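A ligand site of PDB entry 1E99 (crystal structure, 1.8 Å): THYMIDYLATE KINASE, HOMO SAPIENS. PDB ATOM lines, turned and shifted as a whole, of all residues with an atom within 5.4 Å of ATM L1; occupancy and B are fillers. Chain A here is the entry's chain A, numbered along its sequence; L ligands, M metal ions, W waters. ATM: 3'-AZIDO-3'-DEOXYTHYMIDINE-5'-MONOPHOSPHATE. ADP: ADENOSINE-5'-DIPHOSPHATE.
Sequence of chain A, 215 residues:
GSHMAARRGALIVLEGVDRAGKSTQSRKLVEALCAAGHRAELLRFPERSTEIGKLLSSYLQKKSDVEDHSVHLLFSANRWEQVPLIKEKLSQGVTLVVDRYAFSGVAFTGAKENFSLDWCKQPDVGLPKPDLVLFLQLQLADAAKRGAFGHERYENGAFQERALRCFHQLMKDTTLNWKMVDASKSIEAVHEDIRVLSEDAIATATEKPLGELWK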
ATOM      1  N   ASP A  18      11.148  -2.995 -29.429  1.00  0.00           N
ATOM      2  CA  ASP A  18      12.333  -2.375 -28.849  1.00  0.00           C
ATOM      3  C   ASP A  18      13.040  -1.486 -29.865  1.00  0.00           C
ATOM      4  O   ASP A  18      13.159  -1.869 -31.028  1.00  0.00           O
ATOM      5  CB  ASP A  18      13.284  -3.459 -28.319  1.00  0.00           C
ATOM      6  CG  ASP A  18      14.316  -2.872 -27.372  1.00  0.00           C
ATOM      7  OD1 ASP A  18      14.096  -1.841 -26.691  1.00  0.00           O
ATOM      8  OD2 ASP A  18      15.408  -3.438 -27.284  1.00  0.00           O
ATOM      9  N   LYS A  22       9.468   4.768 -29.566  1.00  0.00           N
ATOM     10  CA  LYS A  22       8.337   5.251 -28.758  1.00  0.00           C
ATOM     11  C   LYS A  22       8.645   6.567 -28.077  1.00  0.00           C
ATOM     12  O   LYS A  22       7.872   7.508 -28.046  1.00  0.00           O
ATOM     13  CB  LYS A  22       8.009   4.204 -27.661  1.00  0.00           C
ATOM     14  CG  LYS A  22       7.554   2.881 -28.321  1.00  0.00           C
ATOM     15  CD  LYS A  22       7.320   1.758 -27.315  1.00  0.00           C
ATOM     16  CE  LYS A  22       8.561   1.258 -26.606  1.00  0.00           C
ATOM     17  NZ  LYS A  22       9.590   0.719 -27.555  1.00  0.00           N
ATOM     18  N   SER A  23       9.812   6.656 -27.460  1.00  0.00           N
ATOM     19  CA  SER A  23      10.154   7.838 -26.658  1.00  0.00           C
ATOM     20  C   SER A  23      10.502   9.027 -27.580  1.00  0.00           C
ATOM     21  O   SER A  23       9.976  10.109 -27.333  1.00  0.00           O
ATOM     22  CB  SER A  23      11.310   7.615 -25.699  1.00  0.00           C
ATOM     23  OG  SER A  23      10.970   6.465 -24.888  1.00  0.00           O
ATOM     24  N   PHE A  45       5.119   5.441 -18.955  1.00  0.00           N
ATOM     25  CA  PHE A  45       5.008   4.408 -17.918  1.00  0.00           C
ATOM     26  C   PHE A  45       6.148   3.437 -18.186  1.00  0.00           C
ATOM     27  O   PHE A  45       6.430   3.124 -19.341  1.00  0.00           O
ATOM     28  CB  PHE A  45       3.609   3.784 -17.924  1.00  0.00           C
ATOM     29  CG  PHE A  45       2.564   4.738 -17.412  1.00  0.00           C
ATOM     30  CD1 PHE A  45       2.511   5.012 -16.044  1.00  0.00           C
ATOM     31  CD2 PHE A  45       1.718   5.392 -18.283  1.00  0.00           C
ATOM     32  CE1 PHE A  45       1.542   5.912 -15.591  1.00  0.00           C
ATOM     33  CE2 PHE A  45       0.770   6.271 -17.826  1.00  0.00           C
ATOM     34  CZ  PHE A  45       0.682   6.550 -16.468  1.00  0.00           C
ATOM     35  N   PRO A  46       6.815   2.952 -17.149  1.00  0.00           N
ATOM     36  CA  PRO A  46       6.550   3.324 -15.786  1.00  0.00           C
ATOM     37  C   PRO A  46       6.942   4.770 -15.497  1.00  0.00           C
ATOM     38  O   PRO A  46       7.885   5.305 -16.114  1.00  0.00           O
ATOM     39  CB  PRO A  46       7.510   2.423 -14.974  1.00  0.00           C
ATOM     40  CG  PRO A  46       8.642   2.178 -15.929  1.00  0.00           C
ATOM     41  CD  PRO A  46       7.971   2.032 -17.287  1.00  0.00           C
ATOM     42  N   ARG A  48       8.755   6.639 -13.084  1.00  0.00           N
ATOM     43  CA  ARG A  48       9.678   6.226 -12.019  1.00  0.00           C
ATOM     44  C   ARG A  48       9.855   7.189 -10.876  1.00  0.00           C
ATOM     45  O   ARG A  48      10.654   6.905  -9.965  1.00  0.00           O
ATOM     46  CB  ARG A  48      11.050   6.001 -12.691  1.00  0.00           C
ATOM     47  CG  ARG A  48      10.954   4.978 -13.836  1.00  0.00           C
ATOM     48  CD  ARG A  48      12.368   4.758 -14.384  1.00  0.00           C
ATOM     49  NE  ARG A  48      12.270   3.981 -15.620  1.00  0.00           N
ATOM     50  CZ  ARG A  48      13.174   3.012 -15.860  1.00  0.00           C
ATOM     51  NH1 ARG A  48      14.106   2.798 -14.959  1.00  0.00           N
ATOM     52  NH2 ARG A  48      13.107   2.324 -16.957  1.00  0.00           N
ATOM     53  N   LEU A  60      13.966  -2.825 -12.740  1.00  0.00           N
ATOM     54  CA  LEU A  60      14.343  -2.846 -14.165  1.00  0.00           C
ATOM     55  C   LEU A  60      15.843  -2.716 -14.385  1.00  0.00           C
ATOM     56  O   LEU A  60      16.400  -3.205 -15.370  1.00  0.00           O
ATOM     57  CB  LEU A  60      13.647  -1.704 -14.902  1.00  0.00           C
ATOM     58  CG  LEU A  60      12.143  -1.890 -15.104  1.00  0.00           C
ATOM     59  CD1 LEU A  60      11.545  -0.613 -15.703  1.00  0.00           C
ATOM     60  CD2 LEU A  60      11.853  -3.083 -15.987  1.00  0.00           C
ATOM     61  N   PHE A  75       3.440  -2.370 -11.472  1.00  0.00           N
ATOM     62  CA  PHE A  75       3.394  -1.639 -12.784  1.00  0.00           C
ATOM     63  C   PHE A  75       1.985  -1.108 -13.022  1.00  0.00           C
ATOM     64  O   PHE A  75       1.761   0.007 -13.511  1.00  0.00           O
ATOM     65  CB  PHE A  75       3.824  -2.582 -13.901  1.00  0.00           C
ATOM     66  CG  PHE A  75       5.290  -2.592 -14.232  1.00  0.00           C
ATOM     67  CD1 PHE A  75       5.888  -1.433 -14.763  1.00  0.00           C
ATOM     68  CD2 PHE A  75       6.038  -3.752 -14.040  1.00  0.00           C
ATOM     69  CE1 PHE A  75       7.240  -1.467 -15.090  1.00  0.00           C
ATOM     70  CE2 PHE A  75       7.383  -3.773 -14.384  1.00  0.00           C
ATOM     71  CZ  PHE A  75       7.987  -2.622 -14.871  1.00  0.00           C
ATOM     72  N   SER A  76       0.954  -1.928 -12.743  1.00  0.00           N
ATOM     73  CA  SER A  76      -0.430  -1.486 -12.881  1.00  0.00           C
ATOM     74  C   SER A  76      -0.751  -0.384 -11.873  1.00  0.00           C
ATOM     75  O   SER A  76      -1.391   0.633 -12.196  1.00  0.00           O
ATOM     76  CB  SER A  76      -1.412  -2.655 -12.752  1.00  0.00           C
ATOM     77  OG  SER A  76      -2.730  -2.107 -12.851  1.00  0.00           O
ATOM     78  N   ARG A  79       0.156   3.000 -12.950  1.00  0.00           N
ATOM     79  CA  ARG A  79      -0.771   3.654 -13.862  1.00  0.00           C
ATOM     80  C   ARG A  79      -1.967   4.208 -13.089  1.00  0.00           C
ATOM     81  O   ARG A  79      -2.284   5.380 -13.249  1.00  0.00           O
ATOM     82  CB  ARG A  79      -1.348   2.780 -14.985  1.00  0.00           C
ATOM     83  CG  ARG A  79      -0.217   2.528 -16.018  1.00  0.00           C
ATOM     84  CD  ARG A  79      -0.787   1.497 -17.019  1.00  0.00           C
ATOM     85  NE  ARG A  79      -0.689   0.074 -16.638  1.00  0.00           N
ATOM     86  CZ  ARG A  79       0.420  -0.660 -16.605  1.00  0.00           C
ATOM     87  NH1 ARG A  79       1.654  -0.159 -16.799  1.00  0.00           N
ATOM     88  NH2 ARG A  79       0.280  -1.961 -16.320  1.00  0.00           N
ATOM     89  N   ASP A  99       3.990   7.366 -23.380  1.00  0.00           N
ATOM     90  CA  ASP A  99       5.026   6.450 -23.798  1.00  0.00           C
ATOM     91  C   ASP A  99       4.886   5.149 -23.012  1.00  0.00           C
ATOM     92  O   ASP A  99       5.367   5.136 -21.894  1.00  0.00           O
ATOM     93  CB  ASP A  99       6.378   7.139 -23.496  1.00  0.00           C
ATOM     94  CG  ASP A  99       7.624   6.427 -23.986  1.00  0.00           C
ATOM     95  OD1 ASP A  99       7.530   5.276 -24.470  1.00  0.00           O
ATOM     96  OD2 ASP A  99       8.716   7.023 -23.816  1.00  0.00           O
ATOM     97  N   ARG A 100       4.209   4.173 -23.569  1.00  0.00           N
ATOM     98  CA  ARG A 100       3.869   2.884 -23.012  1.00  0.00           C
ATOM     99  C   ARG A 100       2.637   3.007 -22.074  1.00  0.00           C
ATOM    100  O   ARG A 100       2.520   4.024 -21.385  1.00  0.00           O
ATOM    101  CB  ARG A 100       4.945   2.131 -22.277  1.00  0.00           C
ATOM    102  CG  ARG A 100       6.168   1.764 -23.153  1.00  0.00           C
ATOM    103  CD  ARG A 100       7.018   0.912 -22.154  1.00  0.00           C
ATOM    104  NE  ARG A 100       8.313   0.545 -22.725  1.00  0.00           N
ATOM    105  CZ  ARG A 100       8.544  -0.493 -23.533  1.00  0.00           C
ATOM    106  NH1 ARG A 100       7.615  -1.347 -23.944  1.00  0.00           N
ATOM    107  NH2 ARG A 100       9.803  -0.727 -23.953  1.00  0.00           N
ATOM    108  N   TYR A 101       1.838   1.949 -22.070  1.00  0.00           N
ATOM    109  CA  TYR A 101       0.667   1.973 -21.165  1.00  0.00           C
ATOM    110  C   TYR A 101       0.351   0.552 -20.710  1.00  0.00           C
ATOM    111  O   TYR A 101       1.289  -0.243 -20.535  1.00  0.00           O
ATOM    112  CB  TYR A 101      -0.470   2.672 -21.853  1.00  0.00           C
ATOM    113  CG  TYR A 101      -1.662   3.162 -21.035  1.00  0.00           C
ATOM    114  CD1 TYR A 101      -1.538   4.019 -19.966  1.00  0.00           C
ATOM    115  CD2 TYR A 101      -2.939   2.781 -21.447  1.00  0.00           C
ATOM    116  CE1 TYR A 101      -2.662   4.485 -19.284  1.00  0.00           C
ATOM    117  CE2 TYR A 101      -4.082   3.256 -20.760  1.00  0.00           C
ATOM    118  CZ  TYR A 101      -3.912   4.121 -19.725  1.00  0.00           C
ATOM    119  OH  TYR A 101      -5.036   4.586 -19.042  1.00  0.00           O
ATOM    120  N   SER A 104       1.969  -2.607 -22.621  1.00  0.00           N
ATOM    121  CA  SER A 104       3.322  -3.044 -22.277  1.00  0.00           C
ATOM    122  C   SER A 104       3.195  -3.852 -20.979  1.00  0.00           C
ATOM    123  O   SER A 104       3.836  -4.875 -20.813  1.00  0.00           O
ATOM    124  CB  SER A 104       4.305  -1.881 -22.049  1.00  0.00           C
ATOM    125  OG  SER A 104       4.797  -1.395 -23.309  1.00  0.00           O
ATOM    126  N   GLY A 105       2.331  -3.372 -20.069  1.00  0.00           N
ATOM    127  CA  GLY A 105       2.123  -4.148 -18.830  1.00  0.00           C
ATOM    128  C   GLY A 105       1.832  -5.603 -19.083  1.00  0.00           C
ATOM    129  O   GLY A 105       2.393  -6.512 -18.416  1.00  0.00           O
ATOM    130  N   PHE A 108       4.709  -7.619 -21.304  1.00  0.00           N
ATOM    131  CA  PHE A 108       5.945  -7.968 -20.644  1.00  0.00           C
ATOM    132  C   PHE A 108       5.768  -9.057 -19.596  1.00  0.00           C
ATOM    133  O   PHE A 108       6.603  -9.995 -19.544  1.00  0.00           O
ATOM    134  CB  PHE A 108       6.702  -6.715 -20.155  1.00  0.00           C
ATOM    135  CG  PHE A 108       7.459  -6.146 -21.353  1.00  0.00           C
ATOM    136  CD1 PHE A 108       6.808  -5.309 -22.252  1.00  0.00           C
ATOM    137  CD2 PHE A 108       8.790  -6.459 -21.579  1.00  0.00           C
ATOM    138  CE1 PHE A 108       7.465  -4.817 -23.367  1.00  0.00           C
ATOM    139  CE2 PHE A 108       9.436  -5.939 -22.691  1.00  0.00           C
ATOM    140  CZ  PHE A 108       8.778  -5.122 -23.602  1.00  0.00           C
ATOM    141  N   THR A 109       4.716  -8.964 -18.765  1.00  0.00           N
ATOM    142  CA  THR A 109       4.508 -10.034 -17.779  1.00  0.00           C
ATOM    143  C   THR A 109       4.016 -11.271 -18.518  1.00  0.00           C
ATOM    144  O   THR A 109       4.407 -12.421 -18.242  1.00  0.00           O
ATOM    145  CB  THR A 109       3.510  -9.593 -16.685  1.00  0.00           C
ATOM    146  OG1 THR A 109       4.130  -8.527 -15.958  1.00  0.00           O
ATOM    147  CG2 THR A 109       3.165 -10.737 -15.740  1.00  0.00           C
ATOM    148  N   GLU A 152      19.261  -3.182 -18.975  1.00  0.00           N
ATOM    149  CA  GLU A 152      18.095  -3.299 -18.121  1.00  0.00           C
ATOM    150  C   GLU A 152      17.438  -4.666 -18.316  1.00  0.00           C
ATOM    151  O   GLU A 152      17.686  -5.459 -19.243  1.00  0.00           O
ATOM    152  CB  GLU A 152      17.052  -2.192 -18.331  1.00  0.00           C
ATOM    153  CG  GLU A 152      17.190  -0.842 -17.665  1.00  0.00           C
ATOM    154  CD  GLU A 152      15.980   0.023 -17.343  1.00  0.00           C
ATOM    155  OE1 GLU A 152      14.888   0.040 -17.991  1.00  0.00           O
ATOM    156  OE2 GLU A 152      16.076   0.788 -16.327  1.00  0.00           O
ATOM    157  N   ARG A 153      16.519  -4.979 -17.392  1.00  0.00           N
ATOM    158  CA  ARG A 153      15.774  -6.215 -17.475  1.00  0.00           C
ATOM    159  C   ARG A 153      14.940  -6.232 -18.753  1.00  0.00           C
ATOM    160  O   ARG A 153      14.449  -5.200 -19.212  1.00  0.00           O
ATOM    161  CB  ARG A 153      14.781  -6.278 -16.304  1.00  0.00           C
ATOM    162  CG  ARG A 153      14.699  -7.710 -15.761  1.00  0.00           C
ATOM    163  CD  ARG A 153      13.787  -7.684 -14.540  1.00  0.00           C
ATOM    164  NE  ARG A 153      14.447  -7.302 -13.308  1.00  0.00           N
ATOM    165  CZ  ARG A 153      15.162  -8.083 -12.535  1.00  0.00           C
ATOM    166  NH1 ARG A 153      15.337  -9.337 -12.916  1.00  0.00           N
ATOM    167  NH2 ARG A 153      15.696  -7.697 -11.397  1.00  0.00           N
ATOM    168  N   TYR A 154      14.779  -7.424 -19.285  1.00  0.00           N
ATOM    169  CA  TYR A 154      13.914  -7.708 -20.400  1.00  0.00           C
ATOM    170  C   TYR A 154      14.560  -7.303 -21.747  1.00  0.00           C
ATOM    171  O   TYR A 154      13.955  -7.522 -22.776  1.00  0.00           O
ATOM    172  CB  TYR A 154      12.579  -6.992 -20.251  1.00  0.00           C
ATOM    173  CG  TYR A 154      11.724  -7.203 -19.030  1.00  0.00           C
ATOM    174  CD1 TYR A 154      11.754  -8.418 -18.353  1.00  0.00           C
ATOM    175  CD2 TYR A 154      10.846  -6.223 -18.576  1.00  0.00           C
ATOM    176  CE1 TYR A 154      10.972  -8.653 -17.246  1.00  0.00           C
ATOM    177  CE2 TYR A 154      10.034  -6.455 -17.470  1.00  0.00           C
ATOM    178  CZ  TYR A 154      10.125  -7.677 -16.803  1.00  0.00           C
ATOM    179  OH  TYR A 154       9.311  -7.924 -15.739  1.00  0.00           O
ATOM    180  N   GLU A 155      15.740  -6.715 -21.684  1.00  0.00           N
ATOM    181  CA  GLU A 155      16.362  -6.265 -22.924  1.00  0.00           C
ATOM    182  C   GLU A 155      17.202  -7.350 -23.581  1.00  0.00           C
ATOM    183  O   GLU A 155      18.418  -7.315 -23.555  1.00  0.00           O
ATOM    184  CB  GLU A 155      17.198  -5.017 -22.652  1.00  0.00           C
ATOM    185  CG  GLU A 155      16.261  -3.924 -22.123  1.00  0.00           C
ATOM    186  CD  GLU A 155      16.830  -2.541 -22.358  1.00  0.00           C
ATOM    187  OE1 GLU A 155      17.472  -2.357 -23.410  1.00  0.00           O
ATOM    188  OE2 GLU A 155      16.627  -1.656 -21.520  1.00  0.00           O
ATOM    189  N   GLN A 160      11.925 -10.405 -25.749  1.00  0.00           N
ATOM    190  CA  GLN A 160      11.230  -9.358 -26.536  1.00  0.00           C
ATOM    191  C   GLN A 160      10.278 -10.010 -27.534  1.00  0.00           C
ATOM    192  O   GLN A 160       9.158  -9.607 -27.809  1.00  0.00           O
ATOM    193  CB  GLN A 160      12.244  -8.491 -27.266  1.00  0.00           C
ATOM    194  CG  GLN A 160      13.046  -7.510 -26.430  1.00  0.00           C
ATOM    195  CD  GLN A 160      12.184  -6.329 -26.002  1.00  0.00           C
ATOM    196  OE1 GLN A 160      11.456  -5.782 -26.837  1.00  0.00           O
ATOM    197  NE2 GLN A 160      12.258  -5.960 -24.747  1.00  0.00           N
HETATM  198  P   ATM L   1      11.077   1.801 -21.464  1.00  0.00           P
HETATM  199  OP1 ATM L   1      11.638   0.828 -22.496  1.00  0.00           O
HETATM  200  OP2 ATM L   1       9.881   2.543 -21.904  1.00  0.00           O
HETATM  201  OP3 ATM L   1      12.269   2.507 -20.880  1.00  0.00           O
HETATM  202  O5' ATM L   1      10.439   0.829 -20.303  1.00  0.00           O
HETATM  203  C5' ATM L   1      11.238   0.026 -19.471  1.00  0.00           C
HETATM  204  C4' ATM L   1      10.613  -1.374 -19.223  1.00  0.00           C
HETATM  205  O4' ATM L   1       9.394  -1.583 -18.532  1.00  0.00           O
HETATM  206  C3' ATM L   1      10.486  -2.070 -20.558  1.00  0.00           C
HETATM  207  N3' ATM L   1      11.414  -3.251 -20.510  1.00  0.00           N
HETATM  208  N4' ATM L   1      11.741  -3.650 -21.644  1.00  0.00           N
HETATM  209  N5' ATM L   1      12.329  -3.948 -22.568  1.00  0.00           N
HETATM  210  C2' ATM L   1       8.981  -2.464 -20.631  1.00  0.00           C
HETATM  211  C1' ATM L   1       8.621  -2.576 -19.136  1.00  0.00           C
HETATM  212  N1  ATM L   1       7.228  -2.508 -18.680  1.00  0.00           N
HETATM  213  C2  ATM L   1       6.690  -3.586 -17.956  1.00  0.00           C
HETATM  214  O2  ATM L   1       7.281  -4.654 -17.801  1.00  0.00           O
HETATM  215  N3  ATM L   1       5.424  -3.354 -17.479  1.00  0.00           N
HETATM  216  C4  ATM L   1       4.752  -2.164 -17.670  1.00  0.00           C
HETATM  217  O4  ATM L   1       3.502  -2.024 -17.151  1.00  0.00           O
HETATM  218  C5  ATM L   1       5.386  -1.056 -18.421  1.00  0.00           C
HETATM  219  C5A ATM L   1       4.684   0.234 -18.642  1.00  0.00           C
HETATM  220  C6  ATM L   1       6.654  -1.301 -18.903  1.00  0.00           C
HETATM  221  PB  ADP L   2      12.158   3.279 -27.773  1.00  0.00           P
HETATM  222  O1B ADP L   2      11.086   2.665 -28.619  1.00  0.00           O
HETATM  223  O2B ADP L   2      11.654   4.265 -26.781  1.00  0.00           O
HETATM  224  O3B ADP L   2      13.072   2.213 -27.134  1.00  0.00           O
HETATM  225  PA  ADP L   2      13.908   5.450 -28.745  1.00  0.00           P
HETATM  226  O1A ADP L   2      14.642   5.656 -27.484  1.00  0.00           O
HETATM  227  O2A ADP L   2      12.966   6.528 -29.180  1.00  0.00           O
HETATM  228  O3A ADP L   2      13.130   4.052 -28.829  1.00  0.00           O
HETATM  229  O5' ADP L   2      14.955   5.265 -29.929  1.00  0.00           O
HETATM  230  C5' ADP L   2      15.937   4.208 -29.930  1.00  0.00           C
HETATM  231  C4' ADP L   2      17.195   4.775 -30.639  1.00  0.00           C
HETATM  232  O4' ADP L   2      16.898   4.737 -32.040  1.00  0.00           O
HETATM  233  C3' ADP L   2      17.576   6.201 -30.269  1.00  0.00           C
HETATM  234  O3' ADP L   2      19.003   6.290 -30.366  1.00  0.00           O
HETATM  235  C2' ADP L   2      16.921   7.012 -31.415  1.00  0.00           C
HETATM  236  O2' ADP L   2      17.612   8.182 -31.771  1.00  0.00           O
HETATM  237  C1' ADP L   2      16.975   6.016 -32.590  1.00  0.00           C
HETATM  238  N9  ADP L   2      15.802   6.165 -33.491  1.00  0.00           N
HETATM  239  C8  ADP L   2      14.509   6.368 -33.090  1.00  0.00           C
HETATM  240  N7  ADP L   2      13.668   6.403 -34.119  1.00  0.00           N
HETATM  241  C5  ADP L   2      14.496   6.182 -35.246  1.00  0.00           C
HETATM  242  C6  ADP L   2      14.167   6.120 -36.602  1.00  0.00           C
HETATM  243  N6  ADP L   2      12.974   6.235 -37.084  1.00  0.00           N
HETATM  244  N1  ADP L   2      15.242   5.892 -37.356  1.00  0.00           N
HETATM  245  C2  ADP L   2      16.508   5.747 -36.937  1.00  0.00           C
HETATM  246  N3  ADP L   2      16.882   5.802 -35.656  1.00  0.00           N
HETATM  247  C4  ADP L   2      15.798   6.012 -34.900  1.00  0.00           C
HETATM  248 MG    MG M   1      11.861   4.568 -24.758  1.00  0.00          MG
HETATM  249  O   HOH W   1      11.718   3.613 -18.693  1.00  0.00           O
HETATM  250  O   HOH W   2      13.546  -0.915 -22.697  1.00  0.00           O
HETATM  251  O   HOH W   3      14.146  -2.465 -19.829  1.00  0.00           O
HETATM  252  O   HOH W   4      12.591   2.654 -24.342  1.00  0.00           O
HETATM  253  O   HOH W   5       6.850  -6.846 -16.267  1.00  0.00           O
HETATM  254  O   HOH W   6       8.589   4.312 -20.768  1.00  0.00           O
HETATM  255  O   HOH W   7      14.619   1.913 -20.455  1.00  0.00           O
HETATM  256  O   HOH W   8       9.807   3.837 -24.275  1.00  0.00           O
HETATM  257  O   HOH W   9      11.681  -2.787 -25.456  1.00  0.00           O
HETATM  258  O   HOH W  10      12.045   4.911 -22.656  1.00  0.00           O
HETATM  259  O   HOH W  11       3.915  -5.389 -16.261  1.00  0.00           O
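Residues that only touch ATM L1: Phe 45 (3.4 Å), Pro 46 (3.8 Å), Arg 48 (3.9 Å), Leu 60 (3.7 Å), Phe 75 (3.2 Å), Tyr 101 (3.9 Å), Ser 104 (3.9 Å), Phe 108 (3.2 Å), Glu 152 (3.9 Å), Arg 153 (3.8 Å), Tyr 154 (3.3 Å) and Glu 155 (3.96 Å). Hydrophobic or aromatic side chains that line ATM L1: Phe 45, Pro 46, Leu 60, Phe 75, Phe 108 and Tyr 154.
NH1 of Arg 79 is in hydrogen-bond range of O4 of ATM L1. The guanidinium group (NE) of Arg 100 is in salt-bridge range of an oxygen (OP2) of ATM L1, 2.7 Å away. N5' of ATM L1 sits at hydrogen-bond distance from NE2 of Gln 160. The backbone NH (N) of Gly 105 sits close to an oxygen (O4) of ATM L1 (3.4 Å). N of Ser 23 sits close to O2B of ADP L2 (3.1 Å). An oxygen (O1B) of ADP L2 lies within hydrogen-bond range of the backbone NH (N) of Lys 22 (2.8 Å). The side-chain amino group (NZ) of Lys 22 lies within salt-bridge range of an oxygen (O1B) of ADP L2, 2.7 Å away.
The backbone carbonyl oxygen of Phe 75 lies within hydrogen-bond range of the guanidinium group of Arg 79 (3.3 Å). The guanidinium group (NH1) of Arg 100 is in hydrogen-bond range of the side-chain hydroxyl (OG) of Ser 104, 2.9 Å away. The side-chain amide nitrogen (NE2) of Gln 160 lies within hydrogen-bond range of the backbone carbonyl oxygen (O) of Tyr 154 (3.0 Å). The backbone carbonyl oxygen (O) of Asp 99 sits at hydrogen-bond distance from the backbone NH (N) of Phe 45, 3.0 Å away. The backbone carbonyl oxygen (O) of Leu 60 sits at hydrogen-bond distance from the backbone NH (N) of Arg 153, at 2.7 Å. NH2 of Arg 48 lies within salt-bridge range of OE1 of Glu 152 (3.1 Å).
Water W7 lies within hydrogen-bond range of an oxygen (OP3) of ATM L1 (2.5 Å) and the side-chain carboxylate (OE1) of Glu 152 (3.1 Å). Water W6 lies within hydrogen-bond range of OP2 of ATM L1 (2.5 Å) and O of Phe 45 (2.8 Å). Water W1 bridges an oxygen (OP3) of ATM L1 (2.5 Å) and the guanidinium group of Arg 48 (2.6 Å). Water W8 lies within hydrogen-bond range of OD1 of Asp 99 (2.7 Å) and OP2 of ATM L1 (2.7 Å). Water W4 bridges an oxygen (OP1) of ATM L1 (2.8 Å) and an oxygen (O3B) of ADP L2 (2.9 Å). Water W11 lies within hydrogen-bond range of N3 of ATM L1, O of Gly 105 and OG1 of Thr 109.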
